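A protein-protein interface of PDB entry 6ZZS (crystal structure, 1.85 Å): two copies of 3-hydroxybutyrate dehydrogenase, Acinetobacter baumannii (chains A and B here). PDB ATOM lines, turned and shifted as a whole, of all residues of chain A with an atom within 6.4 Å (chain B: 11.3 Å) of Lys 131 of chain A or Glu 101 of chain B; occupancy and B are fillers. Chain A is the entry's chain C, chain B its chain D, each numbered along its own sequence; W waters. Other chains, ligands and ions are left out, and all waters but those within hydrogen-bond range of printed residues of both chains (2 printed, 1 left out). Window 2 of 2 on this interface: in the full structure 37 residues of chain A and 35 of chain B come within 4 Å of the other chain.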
ATOM      1  N   ILE A 123     -20.302   8.753  -8.404  1.00  0.00           N
ATOM      2  CA  ILE A 123     -20.739   7.848  -9.498  1.00  0.00           C
ATOM      3  C   ILE A 123     -19.666   6.758  -9.642  1.00  0.00           C
ATOM      4  O   ILE A 123     -20.042   5.561  -9.699  1.00  0.00           O
ATOM      5  CB  ILE A 123     -21.017   8.632 -10.797  1.00  0.00           C
ATOM      6  CG1 ILE A 123     -22.295   9.473 -10.675  1.00  0.00           C
ATOM      7  CG2 ILE A 123     -21.065   7.702 -12.002  1.00  0.00           C
ATOM      8  CD1 ILE A 123     -22.561  10.380 -11.858  1.00  0.00           C
ATOM      9  N   LYS A 124     -18.385   7.141  -9.651  1.00  0.00           N
ATOM     10  CA  LYS A 124     -17.268   6.196  -9.923  1.00  0.00           C
ATOM     11  C   LYS A 124     -17.271   5.115  -8.830  1.00  0.00           C
ATOM     12  O   LYS A 124     -17.003   3.954  -9.158  1.00  0.00           O
ATOM     13  CB  LYS A 124     -15.942   6.951 -10.064  1.00  0.00           C
ATOM     14  CG  LYS A 124     -14.690   6.123  -9.822  1.00  0.00           C
ATOM     15  CD  LYS A 124     -13.410   6.933  -9.820  1.00  0.00           C
ATOM     16  CE  LYS A 124     -12.548   6.646 -11.022  1.00  0.00           C
ATOM     17  NZ  LYS A 124     -11.222   7.280 -10.884  1.00  0.00           N
ATOM     18  N   VAL A 126     -19.983   4.172  -6.759  1.00  0.00           N
ATOM     19  CA  VAL A 126     -21.239   3.372  -6.643  1.00  0.00           C
ATOM     20  C   VAL A 126     -21.438   2.533  -7.906  1.00  0.00           C
ATOM     21  O   VAL A 126     -22.110   1.506  -7.810  1.00  0.00           O
ATOM     22  CB  VAL A 126     -22.481   4.220  -6.324  1.00  0.00           C
ATOM     23  CG1 VAL A 126     -22.250   5.049  -5.081  1.00  0.00           C
ATOM     24  CG2 VAL A 126     -22.904   5.089  -7.496  1.00  0.00           C
ATOM     25  N   LEU A 127     -20.850   2.903  -9.045  1.00  0.00           N
ATOM     26  CA  LEU A 127     -21.152   2.167 -10.299  1.00  0.00           C
ATOM     27  C   LEU A 127     -20.831   0.674 -10.157  1.00  0.00           C
ATOM     28  O   LEU A 127     -21.640  -0.133 -10.607  1.00  0.00           O
ATOM     29  CB  LEU A 127     -20.411   2.767 -11.498  1.00  0.00           C
ATOM     30  CG  LEU A 127     -21.146   3.858 -12.275  1.00  0.00           C
ATOM     31  CD1 LEU A 127     -20.324   4.245 -13.497  1.00  0.00           C
ATOM     32  CD2 LEU A 127     -22.544   3.412 -12.695  1.00  0.00           C
ATOM     33  N   PRO A 128     -19.659   0.239  -9.617  1.00  0.00           N
ATOM     34  CA  PRO A 128     -19.331  -1.195  -9.539  1.00  0.00           C
ATOM     35  C   PRO A 128     -20.353  -1.975  -8.698  1.00  0.00           C
ATOM     36  O   PRO A 128     -20.737  -3.065  -9.096  1.00  0.00           O
ATOM     37  CB  PRO A 128     -17.958  -1.252  -8.853  1.00  0.00           C
ATOM     38  CG  PRO A 128     -17.407   0.161  -8.959  1.00  0.00           C
ATOM     39  CD  PRO A 128     -18.607   1.077  -9.013  1.00  0.00           C
ATOM     40  N   ILE A 129     -20.792  -1.384  -7.588  1.00  0.00           N
ATOM     41  CA  ILE A 129     -21.819  -1.958  -6.675  1.00  0.00           C
ATOM     42  C   ILE A 129     -23.143  -2.120  -7.442  1.00  0.00           C
ATOM     43  O   ILE A 129     -23.778  -3.207  -7.367  1.00  0.00           O
ATOM     44  CB  ILE A 129     -22.014  -1.053  -5.446  1.00  0.00           C
ATOM     45  CG1 ILE A 129     -20.703  -0.790  -4.693  1.00  0.00           C
ATOM     46  CG2 ILE A 129     -23.098  -1.611  -4.535  1.00  0.00           C
ATOM     47  CD1 ILE A 129     -20.847   0.187  -3.537  1.00  0.00           C
ATOM     48  N   MET A 130     -23.597  -1.053  -8.108  1.00  0.00           N
ATOM     49  CA  MET A 130     -24.895  -1.058  -8.830  1.00  0.00           C
ATOM     50  C   MET A 130     -24.810  -1.993 -10.037  1.00  0.00           C
ATOM     51  O   MET A 130     -25.852  -2.570 -10.411  1.00  0.00           O
ATOM     52  CB  MET A 130     -25.281   0.350  -9.303  1.00  0.00           C
ATOM     53  CG  MET A 130     -25.754   1.239  -8.175  1.00  0.00           C
ATOM     54  SD  MET A 130     -25.925   2.955  -8.741  1.00  0.00           S
ATOM     55  CE  MET A 130     -26.564   3.658  -7.220  1.00  0.00           C
ATOM     56  N   LYS A 131     -23.652  -2.067 -10.686  1.00  0.00           N
ATOM     57  CA  LYS A 131     -23.486  -2.886 -11.916  1.00  0.00           C
ATOM     58  C   LYS A 131     -23.483  -4.367 -11.528  1.00  0.00           C
ATOM     59  O   LYS A 131     -23.917  -5.185 -12.352  1.00  0.00           O
ATOM     60  CB  LYS A 131     -22.210  -2.538 -12.691  1.00  0.00           C
ATOM     61  CG  LYS A 131     -22.303  -1.265 -13.518  1.00  0.00           C
ATOM     62  CD  LYS A 131     -21.372  -1.241 -14.698  1.00  0.00           C
ATOM     63  CE  LYS A 131     -21.371   0.099 -15.402  1.00  0.00           C
ATOM     64  NZ  LYS A 131     -20.158   0.227 -16.243  1.00  0.00           N
ATOM     65  N   ALA A 132     -22.994  -4.679 -10.334  1.00  0.00           N
ATOM     66  CA  ALA A 132     -22.881  -6.057  -9.810  1.00  0.00           C
ATOM     67  C   ALA A 132     -24.285  -6.576  -9.509  1.00  0.00           C
ATOM     68  O   ALA A 132     -24.532  -7.758  -9.771  1.00  0.00           O
ATOM     69  CB  ALA A 132     -22.001  -6.089  -8.583  1.00  0.00           C
ATOM     70  N   GLN A 133     -25.173  -5.723  -8.996  1.00  0.00           N
ATOM     71  CA  GLN A 133     -26.562  -6.130  -8.648  1.00  0.00           C
ATOM     72  C   GLN A 133     -27.527  -5.858  -9.819  1.00  0.00           C
ATOM     73  O   GLN A 133     -28.708  -6.182  -9.701  1.00  0.00           O
ATOM     74  CB  GLN A 133     -26.994  -5.416  -7.378  1.00  0.00           C
ATOM     75  CG  GLN A 133     -27.298  -3.950  -7.595  1.00  0.00           C
ATOM     76  CD  GLN A 133     -27.696  -3.289  -6.301  1.00  0.00           C
ATOM     77  OE1 GLN A 133     -27.548  -3.861  -5.229  1.00  0.00           O
ATOM     78  NE2 GLN A 133     -28.236  -2.086  -6.391  1.00  0.00           N
ATOM     79  N   LYS A 134     -27.053  -5.253 -10.908  1.00  0.00           N
ATOM     80  CA  LYS A 134     -27.882  -4.916 -12.101  1.00  0.00           C
ATOM     81  C   LYS A 134     -29.081  -4.047 -11.701  1.00  0.00           C
ATOM     82  O   LYS A 134     -30.171  -4.273 -12.262  1.00  0.00           O
ATOM     83  CB  LYS A 134     -28.386  -6.172 -12.818  1.00  0.00           C
ATOM     84  CG  LYS A 134     -27.283  -7.053 -13.369  1.00  0.00           C
ATOM     85  CD  LYS A 134     -26.659  -6.489 -14.597  1.00  0.00           C
ATOM     86  CE  LYS A 134     -25.267  -7.021 -14.824  1.00  0.00           C
ATOM     87  NZ  LYS A 134     -24.767  -6.495 -16.103  1.00  0.00           N
ATOM     88  N   TYR A 135     -28.879  -3.093 -10.787  1.00  0.00           N
ATOM     89  CA  TYR A 135     -29.917  -2.129 -10.345  1.00  0.00           C
ATOM     90  C   TYR A 135     -29.262  -0.894  -9.739  1.00  0.00           C
ATOM     91  O   TYR A 135     -28.434  -1.000  -8.814  1.00  0.00           O
ATOM     92  CB  TYR A 135     -30.889  -2.734  -9.325  1.00  0.00           C
ATOM     93  CG  TYR A 135     -32.089  -1.844  -9.133  1.00  0.00           C
ATOM     94  CD1 TYR A 135     -33.177  -1.916  -9.992  1.00  0.00           C
ATOM     95  CD2 TYR A 135     -32.088  -0.849  -8.168  1.00  0.00           C
ATOM     96  CE1 TYR A 135     -34.257  -1.055  -9.864  1.00  0.00           C
ATOM     97  CE2 TYR A 135     -33.156   0.021  -8.031  1.00  0.00           C
ATOM     98  CZ  TYR A 135     -34.241  -0.089  -8.881  1.00  0.00           C
ATOM     99  OH  TYR A 135     -35.285   0.772  -8.752  1.00  0.00           O
ATOM    100  N   GLU A 173     -23.143   4.529 -20.221  1.00  0.00           N
ATOM    101  CA  GLU A 173     -22.183   3.493 -19.747  1.00  0.00           C
ATOM    102  C   GLU A 173     -22.880   2.435 -18.886  1.00  0.00           C
ATOM    103  O   GLU A 173     -22.294   1.367 -18.739  1.00  0.00           O
ATOM    104  CB  GLU A 173     -21.020   4.109 -18.966  1.00  0.00           C
ATOM    105  CG  GLU A 173     -19.992   4.716 -19.895  1.00  0.00           C
ATOM    106  CD  GLU A 173     -18.822   5.369 -19.197  1.00  0.00           C
ATOM    107  OE1 GLU A 173     -18.557   4.998 -18.010  1.00  0.00           O
ATOM    108  OE2 GLU A 173     -18.186   6.245 -19.842  1.00  0.00           O
ATOM    109  N   CYS A 174     -24.033   2.712 -18.294  1.00  0.00           N
ATOM    110  CA  CYS A 174     -24.735   1.690 -17.472  1.00  0.00           C
ATOM    111  C   CYS A 174     -26.152   1.396 -17.999  1.00  0.00           C
ATOM    112  O   CYS A 174     -26.934   0.737 -17.252  1.00  0.00           O
ATOM    113  CB  CYS A 174     -24.786   2.144 -16.032  1.00  0.00           C
ATOM    114  SG  CYS A 174     -25.684   3.700 -15.843  1.00  0.00           S
ATOM    115  N   ASP A 177     -27.319  -2.110 -17.722  1.00  0.00           N
ATOM    116  CA  ASP A 177     -26.989  -2.689 -16.393  1.00  0.00           C
ATOM    117  C   ASP A 177     -28.105  -2.431 -15.378  1.00  0.00           C
ATOM    118  O   ASP A 177     -27.837  -2.604 -14.199  1.00  0.00           O
ATOM    119  CB  ASP A 177     -25.662  -2.142 -15.846  1.00  0.00           C
ATOM    120  CG  ASP A 177     -24.455  -2.614 -16.624  1.00  0.00           C
ATOM    121  OD1 ASP A 177     -24.402  -3.809 -16.939  1.00  0.00           O
ATOM    122  OD2 ASP A 177     -23.594  -1.779 -16.935  1.00  0.00           O
ATOM    123  N   ILE A 179     -29.401   0.378 -14.468  1.00  0.00           N
ATOM    124  CA  ILE A 179     -29.069   1.660 -13.786  1.00  0.00           C
ATOM    125  C   ILE A 179     -29.554   2.832 -14.646  1.00  0.00           C
ATOM    126  O   ILE A 179     -29.244   2.875 -15.872  1.00  0.00           O
ATOM    127  CB  ILE A 179     -27.558   1.766 -13.521  1.00  0.00           C
ATOM    128  CG1 ILE A 179     -27.022   0.551 -12.764  1.00  0.00           C
ATOM    129  CG2 ILE A 179     -27.240   3.066 -12.811  1.00  0.00           C
ATOM    130  CD1 ILE A 179     -25.515   0.375 -12.834  1.00  0.00           C
ATOM    131  N   HIS B  96      -9.062  12.097 -23.035  1.00  0.00           N
ATOM    132  CA  HIS B  96      -8.770  10.823 -22.332  1.00  0.00           C
ATOM    133  C   HIS B  96     -10.052   9.997 -22.217  1.00  0.00           C
ATOM    134  O   HIS B  96     -10.936  10.384 -21.453  1.00  0.00           O
ATOM    135  CB  HIS B  96      -8.114  11.040 -20.967  1.00  0.00           C
ATOM    136  CG  HIS B  96      -7.633   9.756 -20.363  1.00  0.00           C
ATOM    137  ND1 HIS B  96      -6.350   9.284 -20.562  1.00  0.00           N
ATOM    138  CD2 HIS B  96      -8.264   8.832 -19.598  1.00  0.00           C
ATOM    139  CE1 HIS B  96      -6.210   8.126 -19.949  1.00  0.00           C
ATOM    140  NE2 HIS B  96      -7.375   7.827 -19.347  1.00  0.00           N
ATOM    141  N   VAL B  97     -10.106   8.885 -22.955  1.00  0.00           N
ATOM    142  CA  VAL B  97     -11.268   7.958 -23.064  1.00  0.00           C
ATOM    143  C   VAL B  97     -11.008   6.763 -22.153  1.00  0.00           C
ATOM    144  O   VAL B  97      -9.946   6.139 -22.299  1.00  0.00           O
ATOM    145  CB  VAL B  97     -11.455   7.489 -24.515  1.00  0.00           C
ATOM    146  CG1 VAL B  97     -12.371   6.284 -24.595  1.00  0.00           C
ATOM    147  CG2 VAL B  97     -11.942   8.613 -25.408  1.00  0.00           C
ATOM    148  N   ALA B  98     -11.938   6.480 -21.241  1.00  0.00           N
ATOM    149  CA  ALA B  98     -11.925   5.325 -20.323  1.00  0.00           C
ATOM    150  C   ALA B  98     -13.312   5.190 -19.714  1.00  0.00           C
ATOM    151  O   ALA B  98     -13.983   6.198 -19.538  1.00  0.00           O
ATOM    152  CB  ALA B  98     -10.899   5.540 -19.247  1.00  0.00           C
ATOM    153  N   PRO B  99     -13.795   3.959 -19.419  1.00  0.00           N
ATOM    154  CA  PRO B  99     -15.000   3.781 -18.626  1.00  0.00           C
ATOM    155  C   PRO B  99     -14.832   4.610 -17.369  1.00  0.00           C
ATOM    156  O   PRO B  99     -13.715   4.674 -16.893  1.00  0.00           O
ATOM    157  CB  PRO B  99     -15.010   2.293 -18.256  1.00  0.00           C
ATOM    158  CG  PRO B  99     -14.231   1.639 -19.365  1.00  0.00           C
ATOM    159  CD  PRO B  99     -13.230   2.672 -19.845  1.00  0.00           C
ATOM    160  N   ILE B 100     -15.931   5.096 -16.806  1.00  0.00           N
ATOM    161  CA  ILE B 100     -15.896   5.908 -15.556  1.00  0.00           C
ATOM    162  C   ILE B 100     -15.094   5.182 -14.467  1.00  0.00           C
ATOM    163  O   ILE B 100     -14.326   5.885 -13.730  1.00  0.00           O
ATOM    164  CB  ILE B 100     -17.305   6.318 -15.094  1.00  0.00           C
ATOM    165  CG1 ILE B 100     -17.894   7.369 -16.038  1.00  0.00           C
ATOM    166  CG2 ILE B 100     -17.279   6.830 -13.653  1.00  0.00           C
ATOM    167  CD1 ILE B 100     -19.335   7.701 -15.742  1.00  0.00           C
ATOM    168  N   GLU B 101     -15.258   3.860 -14.300  1.00  0.00           N
ATOM    169  CA  GLU B 101     -14.633   3.156 -13.140  1.00  0.00           C
ATOM    170  C   GLU B 101     -13.104   3.168 -13.269  1.00  0.00           C
ATOM    171  O   GLU B 101     -12.465   3.185 -12.225  1.00  0.00           O
ATOM    172  CB  GLU B 101     -15.155   1.731 -12.955  1.00  0.00           C
ATOM    173  CG  GLU B 101     -16.652   1.671 -12.728  1.00  0.00           C
ATOM    174  CD  GLU B 101     -17.422   1.347 -13.993  1.00  0.00           C
ATOM    175  OE1 GLU B 101     -17.094   1.934 -15.065  1.00  0.00           O
ATOM    176  OE2 GLU B 101     -18.330   0.496 -13.912  1.00  0.00           O
ATOM    177  N   GLU B 102     -12.555   3.177 -14.486  1.00  0.00           N
ATOM    178  CA  GLU B 102     -11.095   3.203 -14.774  1.00  0.00           C
ATOM    179  C   GLU B 102     -10.621   4.615 -15.155  1.00  0.00           C
ATOM    180  O   GLU B 102      -9.463   4.729 -15.625  1.00  0.00           O
ATOM    181  CB  GLU B 102     -10.774   2.246 -15.926  1.00  0.00           C
ATOM    182  CG  GLU B 102     -11.058   0.781 -15.608  1.00  0.00           C
ATOM    183  CD  GLU B 102     -11.346  -0.078 -16.833  1.00  0.00           C
ATOM    184  OE1 GLU B 102     -10.725   0.168 -17.902  1.00  0.00           O
ATOM    185  OE2 GLU B 102     -12.207  -0.985 -16.729  1.00  0.00           O
ATOM    186  N   PHE B 103     -11.469   5.637 -14.977  1.00  0.00           N
ATOM    187  CA  PHE B 103     -11.218   7.060 -15.350  1.00  0.00           C
ATOM    188  C   PHE B 103     -10.549   7.749 -14.161  1.00  0.00           C
ATOM    189  O   PHE B 103     -11.209   8.009 -13.158  1.00  0.00           O
ATOM    190  CB  PHE B 103     -12.515   7.781 -15.763  1.00  0.00           C
ATOM    191  CG  PHE B 103     -12.293   8.935 -16.715  1.00  0.00           C
ATOM    192  CD1 PHE B 103     -11.584  10.063 -16.318  1.00  0.00           C
ATOM    193  CD2 PHE B 103     -12.744   8.877 -18.024  1.00  0.00           C
ATOM    194  CE1 PHE B 103     -11.343  11.104 -17.203  1.00  0.00           C
ATOM    195  CE2 PHE B 103     -12.521   9.930 -18.905  1.00  0.00           C
ATOM    196  CZ  PHE B 103     -11.836  11.049 -18.488  1.00  0.00           C
ATOM    197  N   PRO B 104      -9.225   8.034 -14.187  1.00  0.00           N
ATOM    198  CA  PRO B 104      -8.581   8.618 -13.016  1.00  0.00           C
ATOM    199  C   PRO B 104      -9.216   9.997 -12.763  1.00  0.00           C
ATOM    200  O   PRO B 104      -9.404  10.769 -13.713  1.00  0.00           O
ATOM    201  CB  PRO B 104      -7.093   8.697 -13.361  1.00  0.00           C
ATOM    202  CG  PRO B 104      -6.939   7.919 -14.647  1.00  0.00           C
ATOM    203  CD  PRO B 104      -8.295   7.903 -15.322  1.00  0.00           C
ATOM    204  N   THR B 105      -9.573  10.237 -11.503  1.00  0.00           N
ATOM    205  CA  THR B 105     -10.150  11.503 -11.013  1.00  0.00           C
ATOM    206  C   THR B 105      -9.293  12.694 -11.439  1.00  0.00           C
ATOM    207  O   THR B 105      -9.884  13.709 -11.854  1.00  0.00           O
ATOM    208  CB  THR B 105     -10.322  11.468  -9.504  1.00  0.00           C
ATOM    209  OG1 THR B 105     -11.032  10.261  -9.228  1.00  0.00           O
ATOM    210  CG2 THR B 105     -11.072  12.675  -9.003  1.00  0.00           C
ATOM    211  N   ALA B 106      -7.972  12.597 -11.290  1.00  0.00           N
ATOM    212  CA  ALA B 106      -7.039  13.691 -11.621  1.00  0.00           C
ATOM    213  C   ALA B 106      -7.128  13.997 -13.122  1.00  0.00           C
ATOM    214  O   ALA B 106      -7.070  15.184 -13.474  1.00  0.00           O
ATOM    215  CB  ALA B 106      -5.628  13.351 -11.185  1.00  0.00           C
ATOM    216  N   VAL B 107      -7.270  12.976 -13.969  1.00  0.00           N
ATOM    217  CA  VAL B 107      -7.369  13.153 -15.444  1.00  0.00           C
ATOM    218  C   VAL B 107      -8.721  13.819 -15.736  1.00  0.00           C
ATOM    219  O   VAL B 107      -8.759  14.732 -16.590  1.00  0.00           O
ATOM    220  CB  VAL B 107      -7.181  11.835 -16.210  1.00  0.00           C
ATOM    221  CG1 VAL B 107      -7.464  12.006 -17.701  1.00  0.00           C
ATOM    222  CG2 VAL B 107      -5.795  11.247 -15.996  1.00  0.00           C
ATOM    223  N   PHE B 108      -9.775  13.431 -15.017  1.00  0.00           N
ATOM    224  CA  PHE B 108     -11.104  14.090 -15.105  1.00  0.00           C
ATOM    225  C   PHE B 108     -10.933  15.580 -14.753  1.00  0.00           C
ATOM    226  O   PHE B 108     -11.490  16.457 -15.471  1.00  0.00           O
ATOM    227  CB  PHE B 108     -12.116  13.426 -14.166  1.00  0.00           C
ATOM    228  CG  PHE B 108     -13.479  14.072 -14.165  1.00  0.00           C
ATOM    229  CD1 PHE B 108     -13.744  15.174 -13.371  1.00  0.00           C
ATOM    230  CD2 PHE B 108     -14.483  13.606 -15.006  1.00  0.00           C
ATOM    231  CE1 PHE B 108     -14.991  15.780 -13.396  1.00  0.00           C
ATOM    232  CE2 PHE B 108     -15.736  14.206 -15.023  1.00  0.00           C
ATOM    233  CZ  PHE B 108     -15.991  15.294 -14.219  1.00  0.00           C
ATOM    234  N   ALA B 151     -20.193   7.349 -24.319  1.00  0.00           N
ATOM    235  CA  ALA B 151     -19.631   6.447 -23.286  1.00  0.00           C
ATOM    236  C   ALA B 151     -18.093   6.516 -23.336  1.00  0.00           C
ATOM    237  O   ALA B 151     -17.551   6.520 -24.431  1.00  0.00           O
ATOM    238  CB  ALA B 151     -20.140   5.041 -23.486  1.00  0.00           C
ATOM    239  N   GLY B 152     -17.442   6.630 -22.178  1.00  0.00           N
ATOM    240  CA  GLY B 152     -15.977   6.722 -22.013  1.00  0.00           C
ATOM    241  C   GLY B 152     -15.445   8.154 -21.998  1.00  0.00           C
ATOM    242  O   GLY B 152     -14.215   8.309 -21.870  1.00  0.00           O
ATOM    243  N   LYS B 153     -16.295   9.172 -22.163  1.00  0.00           N
ATOM    244  CA  LYS B 153     -15.826  10.579 -22.320  1.00  0.00           C
ATOM    245  C   LYS B 153     -16.358  11.420 -21.165  1.00  0.00           C
ATOM    246  O   LYS B 153     -16.694  12.614 -21.394  1.00  0.00           O
ATOM    247  CB  LYS B 153     -16.214  11.119 -23.702  1.00  0.00           C
ATOM    248  CG  LYS B 153     -15.230  10.776 -24.812  1.00  0.00           C
ATOM    249  CD  LYS B 153     -15.693  11.067 -26.215  1.00  0.00           C
ATOM    250  CE  LYS B 153     -14.978  10.170 -27.205  1.00  0.00           C
ATOM    251  NZ  LYS B 153     -15.167  10.579 -28.613  1.00  0.00           N
ATOM    252  N   ALA B 154     -16.422  10.843 -19.966  1.00  0.00           N
ATOM    253  CA  ALA B 154     -16.948  11.533 -18.763  1.00  0.00           C
ATOM    254  C   ALA B 154     -16.285  12.912 -18.603  1.00  0.00           C
ATOM    255  O   ALA B 154     -16.978  13.895 -18.332  1.00  0.00           O
ATOM    256  CB  ALA B 154     -16.732  10.694 -17.539  1.00  0.00           C
ATOM    257  N   GLY B 155     -14.966  12.977 -18.732  1.00  0.00           N
ATOM    258  CA  GLY B 155     -14.225  14.216 -18.454  1.00  0.00           C
ATOM    259  C   GLY B 155     -14.428  15.219 -19.560  1.00  0.00           C
ATOM    260  O   GLY B 155     -14.725  16.365 -19.245  1.00  0.00           O
HETATM  261  O   HOH W   1     -18.828   2.535 -16.707  1.00  0.00           O
HETATM  262  O   HOH W   2      -8.343   8.209  -9.564  1.00  0.00           O
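The backbone carbonyl oxygen (O) of Glu 173 of chain A lies within hydrogen-bond range of the side-chain amino group (NZ) of Lys 131 of chain A, 3.5 Å away. The backbone NH (N) of Ala 98 of chain B is in hydrogen-bond range of the backbone carbonyl oxygen (O) of Gly 152 of chain B, 3.0 Å away.
Printed residues of chain B that touch a printed residue of chain A: Pro 99, Ile 100, Glu 101, Phe 103, Pro 104, Thr 105, Ala 151 and Gly 152. Hydrophobic or aromatic side chains of chain A that line the printed part of chain B: Leu 127. Among the printed residues, 12 pairs touch across the chains. Among the printed residues, Asp or Glu carboxylates within 4 Å of a Lys or Arg side-chain nitrogen of the other chain: Lys 131 of chain A with Glu 101 of chain B (3.0 Å).
Water W1 lies within hydrogen-bond range of the side-chain carboxylate (OE1) of Glu 101 of chain B (2.5 Å), the side-chain amino group (NZ) of Lys 131 of chain A (2.7 Å) and the side-chain carboxylate (OE1) of Glu 173 of chain A (2.8 Å). Water W2 lies within hydrogen-bond range of the backbone NH of Thr 105 of chain B (3.1 Å) and the side-chain amino group of Lys 124 of chain A (3.3 Å).
Lys 124 of chain A touches Ile 100 of chain B. CE of Lys 124 of chain A touches O of Glu 101 of chain B (3.7 Å). NZ of Lys 124 of chain A touches CA of Pro 104 of chain B, at 3.6 Å. Leu 127 of chain A touches Ile 100 of chain B. Leu 127 of chain A touches Glu 101 of chain B (CB to OE2, 3.9 Å). Pro 99 of chain B touches Glu 173 of chain A. Glu 173 of chain A touches Ala 151 of chain B (OE2 to C, 3.5 Å).
No position is printed for both chains. Of the 12 pairs that touch across the chains among the printed residues, none has its exchanged pair printed and touching as well.
The side-chain amino group (NZ) of Lys 124 of chain A lies within hydrogen-bond range of the side-chain hydroxyl (OG1) of Thr 105 of chain B, 3.4 Å away. The side-chain amino group of Lys 131 of chain A is in salt-bridge range of the side-chain carboxylate of Glu 101 of chain B (3.0 Å). The backbone NH of Ile 100 of chain B is in hydrogen-bond range of the side-chain carboxylate of Glu 173 of chain A (2.9 Å). OE2 of Glu 173 of chain A sits at hydrogen-bond distance from N of Gly 152 of chain B (2.5 Å). The side-chain amino group (NZ) of Lys 124 of chain A lies close to the backbone carbonyl oxygen (O) of Phe 103 of chain B.
Lys 124 of chain A touches just these residues of chain B: Ile 100, Glu 101, Phe 103, Pro 104 and Thr 105. Printed residues of chain B within 4 Å of Leu 127 of chain A: Ile 100 (3.995 Å) and Glu 101 (3.9 Å). No residue of chain B comes within 4 Å of Pro 128 of chain A. Of chain B, only Glu 101 comes within 4 Å of Lys 131 of chain A. Ala 132 of chain A touches none of the printed residues of chain B. Gln 133 of chain A touches none of the printed residues of chain B. No residue of chain B comes within 4 Å of Lys 134 of chain A. Printed residues of chain B within 4 Å of Glu 173 of chain A: Pro 99, Ile 100, Ala 151 and Gly 152. No residue of chain B comes within 4 Å of Cys 174 of chain A. Printed residues of chain A within 4 Å of Pro 99 of chain B: Glu 173. Printed residues of chain A within 4 Å of Ile 100 of chain B: Lys 124, Leu 127 and Glu 173. Glu 101 of chain B touches just these residues of chain A: Lys 124, Leu 127 and Lys 131. Of the printed residues of chain A, Ala 151 of chain B touches Glu 173. The nearest residue of chain B that does not touch Lys 131 of chain A is Pro 99 of chain B (5.9 Å). The nearest residue of chain A that does not touch Glu 101 of chain B is Pro 128 of chain A (4.1 Å).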
